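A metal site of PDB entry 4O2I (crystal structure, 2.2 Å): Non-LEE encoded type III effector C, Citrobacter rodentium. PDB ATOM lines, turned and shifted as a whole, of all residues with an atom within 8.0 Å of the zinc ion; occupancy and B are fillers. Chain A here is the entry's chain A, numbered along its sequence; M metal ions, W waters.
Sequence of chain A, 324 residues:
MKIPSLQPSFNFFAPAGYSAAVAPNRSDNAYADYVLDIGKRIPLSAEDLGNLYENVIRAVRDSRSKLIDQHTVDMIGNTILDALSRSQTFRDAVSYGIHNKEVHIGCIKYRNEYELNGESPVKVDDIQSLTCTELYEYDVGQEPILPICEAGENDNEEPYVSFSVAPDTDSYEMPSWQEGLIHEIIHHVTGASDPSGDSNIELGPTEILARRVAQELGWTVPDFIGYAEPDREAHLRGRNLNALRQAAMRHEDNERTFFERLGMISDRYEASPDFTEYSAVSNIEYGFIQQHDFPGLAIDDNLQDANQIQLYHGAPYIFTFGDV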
ATOM      1  N   CYS A 149      -4.874 -20.460  14.802  1.00  0.00           N
ATOM      2  CA  CYS A 149      -6.118 -20.007  15.390  1.00  0.00           C
ATOM      3  C   CYS A 149      -5.799 -18.867  16.360  1.00  0.00           C
ATOM      4  O   CYS A 149      -5.259 -19.095  17.443  1.00  0.00           O
ATOM      5  CB  CYS A 149      -6.845 -21.173  16.077  1.00  0.00           C
ATOM      6  SG  CYS A 149      -7.270 -22.524  14.947  1.00  0.00           S
ATOM      7  N   GLU A 150      -6.121 -17.646  15.950  1.00  0.00           N
ATOM      8  CA  GLU A 150      -5.778 -16.459  16.726  1.00  0.00           C
ATOM      9  C   GLU A 150      -6.570 -15.213  16.326  1.00  0.00           C
ATOM     10  O   GLU A 150      -7.109 -15.126  15.219  1.00  0.00           O
ATOM     11  CB  GLU A 150      -4.273 -16.157  16.640  1.00  0.00           C
ATOM     12  CG  GLU A 150      -3.838 -15.646  15.277  1.00  0.00           C
ATOM     13  CD  GLU A 150      -2.370 -15.276  15.207  1.00  0.00           C
ATOM     14  OE1 GLU A 150      -1.628 -15.544  16.179  1.00  0.00           O
ATOM     15  OE2 GLU A 150      -1.950 -14.733  14.161  1.00  0.00           O
ATOM     16  N   ALA A 151      -6.612 -14.273  17.250  1.00  0.00           N
ATOM     17  CA  ALA A 151      -7.198 -12.970  17.029  1.00  0.00           C
ATOM     18  C   ALA A 151      -6.033 -11.999  17.009  1.00  0.00           C
ATOM     19  O   ALA A 151      -5.402 -11.752  18.043  1.00  0.00           O
ATOM     20  CB  ALA A 151      -8.155 -12.633  18.166  1.00  0.00           C
ATOM     21  N   GLY A 180     -15.257 -22.519  18.510  1.00  0.00           N
ATOM     22  CA  GLY A 180     -13.892 -21.985  18.388  1.00  0.00           C
ATOM     23  C   GLY A 180     -13.792 -20.699  17.566  1.00  0.00           C
ATOM     24  O   GLY A 180     -12.977 -19.831  17.869  1.00  0.00           O
ATOM     25  N   HIS A 183     -15.050 -18.047  19.842  1.00  0.00           N
ATOM     26  CA  HIS A 183     -13.992 -17.790  20.812  1.00  0.00           C
ATOM     27  C   HIS A 183     -13.036 -16.720  20.320  1.00  0.00           C
ATOM     28  O   HIS A 183     -12.794 -15.738  21.021  1.00  0.00           O
ATOM     29  CB  HIS A 183     -13.263 -19.088  21.127  1.00  0.00           C
ATOM     30  CG  HIS A 183     -12.003 -18.896  21.940  1.00  0.00           C
ATOM     31  ND1 HIS A 183     -11.937 -19.226  23.254  1.00  0.00           N
ATOM     32  CD2 HIS A 183     -10.749 -18.408  21.599  1.00  0.00           C
ATOM     33  CE1 HIS A 183     -10.702 -18.954  23.706  1.00  0.00           C
ATOM     34  NE2 HIS A 183      -9.982 -18.445  22.692  1.00  0.00           N
ATOM     35  N   GLU A 184     -12.503 -16.883  19.111  1.00  0.00           N
ATOM     36  CA  GLU A 184     -11.523 -15.929  18.584  1.00  0.00           C
ATOM     37  C   GLU A 184     -12.104 -14.533  18.424  1.00  0.00           C
ATOM     38  O   GLU A 184     -11.426 -13.523  18.694  1.00  0.00           O
ATOM     39  CB  GLU A 184     -10.901 -16.434  17.271  1.00  0.00           C
ATOM     40  CG  GLU A 184     -10.247 -17.815  17.340  1.00  0.00           C
ATOM     41  CD  GLU A 184      -9.122 -17.914  18.375  1.00  0.00           C
ATOM     42  OE1 GLU A 184      -8.637 -16.876  18.884  1.00  0.00           O
ATOM     43  OE2 GLU A 184      -8.710 -19.050  18.688  1.00  0.00           O
ATOM     44  N   ILE A 185     -13.373 -14.463  18.005  1.00  0.00           N
ATOM     45  CA  ILE A 185     -14.074 -13.200  17.814  1.00  0.00           C
ATOM     46  C   ILE A 185     -14.251 -12.491  19.159  1.00  0.00           C
ATOM     47  O   ILE A 185     -14.157 -11.272  19.255  1.00  0.00           O
ATOM     48  CB  ILE A 185     -15.438 -13.419  17.154  1.00  0.00           C
ATOM     49  CG1 ILE A 185     -15.253 -13.851  15.685  1.00  0.00           C
ATOM     50  CG2 ILE A 185     -16.290 -12.153  17.220  1.00  0.00           C
ATOM     51  CD1 ILE A 185     -16.505 -14.394  15.030  1.00  0.00           C
ATOM     52  N   ILE A 186     -14.474 -13.274  20.212  1.00  0.00           N
ATOM     53  CA  ILE A 186     -14.624 -12.720  21.539  1.00  0.00           C
ATOM     54  C   ILE A 186     -13.346 -12.029  22.056  1.00  0.00           C
ATOM     55  O   ILE A 186     -13.436 -10.985  22.722  1.00  0.00           O
ATOM     56  CB  ILE A 186     -15.219 -13.757  22.519  1.00  0.00           C
ATOM     57  CG1 ILE A 186     -16.723 -13.851  22.273  1.00  0.00           C
ATOM     58  CG2 ILE A 186     -14.925 -13.375  23.960  1.00  0.00           C
ATOM     59  CD1 ILE A 186     -17.389 -15.077  22.832  1.00  0.00           C
ATOM     60  N   HIS A 187     -12.176 -12.570  21.713  1.00  0.00           N
ATOM     61  CA  HIS A 187     -10.914 -11.865  21.997  1.00  0.00           C
ATOM     62  C   HIS A 187     -10.944 -10.421  21.542  1.00  0.00           C
ATOM     63  O   HIS A 187     -10.582  -9.537  22.303  1.00  0.00           O
ATOM     64  CB  HIS A 187      -9.719 -12.550  21.345  1.00  0.00           C
ATOM     65  CG  HIS A 187      -9.209 -13.742  22.114  1.00  0.00           C
ATOM     66  ND1 HIS A 187      -8.884 -13.682  23.417  1.00  0.00           N
ATOM     67  CD2 HIS A 187      -8.937 -15.043  21.695  1.00  0.00           C
ATOM     68  CE1 HIS A 187      -8.439 -14.887  23.829  1.00  0.00           C
ATOM     69  NE2 HIS A 187      -8.466 -15.715  22.775  1.00  0.00           N
ATOM     70  N   ALA A 192     -11.096  -9.646  26.100  1.00  0.00           N
ATOM     71  CA  ALA A 192     -10.787 -10.750  27.022  1.00  0.00           C
ATOM     72  C   ALA A 192      -9.592 -11.570  26.547  1.00  0.00           C
ATOM     73  O   ALA A 192      -9.330 -11.669  25.345  1.00  0.00           O
ATOM     74  CB  ALA A 192     -11.997 -11.653  27.221  1.00  0.00           C
ATOM     75  N   SER A 193      -8.895 -12.172  27.493  1.00  0.00           N
ATOM     76  CA  SER A 193      -7.694 -12.944  27.201  1.00  0.00           C
ATOM     77  C   SER A 193      -7.859 -14.430  27.586  1.00  0.00           C
ATOM     78  O   SER A 193      -8.848 -14.807  28.225  1.00  0.00           O
ATOM     79  CB  SER A 193      -6.507 -12.318  27.917  1.00  0.00           C
ATOM     80  OG  SER A 193      -5.336 -12.410  27.129  1.00  0.00           O
ATOM     81  N   ASP A 194      -6.909 -15.261  27.181  1.00  0.00           N
ATOM     82  CA  ASP A 194      -6.831 -16.635  27.650  1.00  0.00           C
ATOM     83  C   ASP A 194      -6.006 -16.680  28.934  1.00  0.00           C
ATOM     84  O   ASP A 194      -5.270 -15.741  29.224  1.00  0.00           O
ATOM     85  CB  ASP A 194      -6.239 -17.544  26.573  1.00  0.00           C
ATOM     86  CG  ASP A 194      -7.177 -17.721  25.377  1.00  0.00           C
ATOM     87  OD1 ASP A 194      -8.413 -17.811  25.573  1.00  0.00           O
ATOM     88  OD2 ASP A 194      -6.666 -17.778  24.238  1.00  0.00           O
ATOM     89  N   PRO A 195      -6.133 -17.774  29.722  1.00  0.00           N
ATOM     90  CA  PRO A 195      -5.415 -17.844  31.002  1.00  0.00           C
ATOM     91  C   PRO A 195      -3.914 -17.586  30.883  1.00  0.00           C
ATOM     92  O   PRO A 195      -3.291 -17.928  29.874  1.00  0.00           O
ATOM     93  CB  PRO A 195      -5.680 -19.272  31.465  1.00  0.00           C
ATOM     94  CG  PRO A 195      -7.009 -19.593  30.879  1.00  0.00           C
ATOM     95  CD  PRO A 195      -7.027 -18.930  29.541  1.00  0.00           C
ATOM     96  N   LEU A 203     -11.023 -22.241  32.408  1.00  0.00           N
ATOM     97  CA  LEU A 203     -11.134 -22.028  30.973  1.00  0.00           C
ATOM     98  C   LEU A 203     -10.616 -20.654  30.553  1.00  0.00           C
ATOM     99  O   LEU A 203     -10.171 -20.478  29.413  1.00  0.00           O
ATOM    100  CB  LEU A 203     -12.594 -22.187  30.520  1.00  0.00           C
ATOM    101  CG  LEU A 203     -13.234 -23.574  30.653  1.00  0.00           C
ATOM    102  CD1 LEU A 203     -14.734 -23.503  30.377  1.00  0.00           C
ATOM    103  CD2 LEU A 203     -12.564 -24.594  29.734  1.00  0.00           C
ATOM    104  N   THR A 206     -12.440 -15.770  27.961  1.00  0.00           N
ATOM    105  CA  THR A 206     -12.769 -15.892  26.536  1.00  0.00           C
ATOM    106  C   THR A 206     -13.499 -17.217  26.250  1.00  0.00           C
ATOM    107  O   THR A 206     -14.532 -17.231  25.558  1.00  0.00           O
ATOM    108  CB  THR A 206     -11.509 -15.754  25.634  1.00  0.00           C
ATOM    109  OG1 THR A 206     -10.768 -14.579  25.995  1.00  0.00           O
ATOM    110  CG2 THR A 206     -11.901 -15.645  24.173  1.00  0.00           C
ATOM    111  N   GLU A 207     -12.984 -18.312  26.796  1.00  0.00           N
ATOM    112  CA  GLU A 207     -13.606 -19.625  26.625  1.00  0.00           C
ATOM    113  C   GLU A 207     -14.945 -19.736  27.366  1.00  0.00           C
ATOM    114  O   GLU A 207     -15.891 -20.314  26.835  1.00  0.00           O
ATOM    115  CB  GLU A 207     -12.645 -20.751  27.003  1.00  0.00           C
ATOM    116  CG  GLU A 207     -13.146 -22.168  26.691  1.00  0.00           C
ATOM    117  CD  GLU A 207     -13.524 -22.411  25.224  1.00  0.00           C
ATOM    118  OE1 GLU A 207     -13.165 -21.583  24.347  1.00  0.00           O
ATOM    119  OE2 GLU A 207     -14.188 -23.430  24.952  1.00  0.00           O
ATOM    120  N   TYR A 227      -8.391 -24.634  29.985  1.00  0.00           N
ATOM    121  CA  TYR A 227      -8.041 -24.180  28.636  1.00  0.00           C
ATOM    122  C   TYR A 227      -6.898 -24.988  28.020  1.00  0.00           C
ATOM    123  O   TYR A 227      -6.835 -25.153  26.803  1.00  0.00           O
ATOM    124  CB  TYR A 227      -7.675 -22.676  28.623  1.00  0.00           C
ATOM    125  CG  TYR A 227      -7.586 -22.064  27.230  1.00  0.00           C
ATOM    126  CD1 TYR A 227      -8.741 -21.857  26.464  1.00  0.00           C
ATOM    127  CD2 TYR A 227      -6.357 -21.713  26.673  1.00  0.00           C
ATOM    128  CE1 TYR A 227      -8.668 -21.305  25.198  1.00  0.00           C
ATOM    129  CE2 TYR A 227      -6.274 -21.155  25.394  1.00  0.00           C
ATOM    130  CZ  TYR A 227      -7.436 -20.962  24.662  1.00  0.00           C
ATOM    131  OH  TYR A 227      -7.383 -20.409  23.389  1.00  0.00           O
ATOM    132  N   ARG A 232      -8.455 -31.326  26.152  1.00  0.00           N
ATOM    133  CA  ARG A 232      -8.851 -30.223  25.279  1.00  0.00           C
ATOM    134  C   ARG A 232      -7.894 -30.098  24.098  1.00  0.00           C
ATOM    135  O   ARG A 232      -8.329 -30.027  22.946  1.00  0.00           O
ATOM    136  CB  ARG A 232      -8.985 -28.905  26.049  1.00  0.00           C
ATOM    137  CG  ARG A 232      -9.568 -27.792  25.200  1.00  0.00           C
ATOM    138  CD  ARG A 232     -10.013 -26.588  26.006  1.00  0.00           C
ATOM    139  NE  ARG A 232     -10.575 -25.582  25.101  1.00  0.00           N
ATOM    140  CZ  ARG A 232      -9.861 -24.695  24.409  1.00  0.00           C
ATOM    141  NH1 ARG A 232      -8.535 -24.652  24.521  1.00  0.00           N
ATOM    142  NH2 ARG A 232     -10.476 -23.843  23.599  1.00  0.00           N
HETATM  143 ZN    ZN M   1      -8.124 -17.689  22.860  1.00  0.00          ZN
HETATM  144  O   HOH W   1      -7.137 -18.060  21.334  1.00  0.00           O
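A ring nitrogen (ND1) of His 187 lies close to the side-chain hydroxyl (OG1) of Thr 206 (3.3 Å). A ring nitrogen (ND1) of His 187 is in hydrogen-bond range of the backbone carbonyl oxygen of Ala 192 (2.8 Å). The side-chain carboxylate (OD2) of Asp 194 sits close to the side-chain hydroxyl (OH) of Tyr 227 (2.9 Å). A ring nitrogen (NE2) of His 183 lies close to the side-chain hydroxyl of Tyr 227 (3.3 Å). A ring nitrogen (ND1) of His 183 lies within hydrogen-bond range of the side-chain carboxylate of Glu 207, at 2.9 Å. The guanidinium group (NH1) of Arg 232 lies within hydrogen-bond range of the backbone carbonyl oxygen (O) of Tyr 227 (2.9 Å).
Water W1 lies within hydrogen-bond range of the side-chain carboxylate of Glu 184 and the side-chain hydroxyl of Tyr 227.
The zinc ion is bound by water W1 (1.9 Å), a ring nitrogen (NE2) of His 187 (2.0 Å), the side-chain carboxylate of Asp 194 (2.0 Å) and a ring nitrogen (NE2) of His 183 (2.0 Å). Slightly farther from the zinc ion lies OD1 of Asp 194 (2.7 Å).
Residues that only touch the zinc ion: Tyr 227. The nearest printed residue that does not touch the zinc ion is Glu 184 (4.1 Å).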
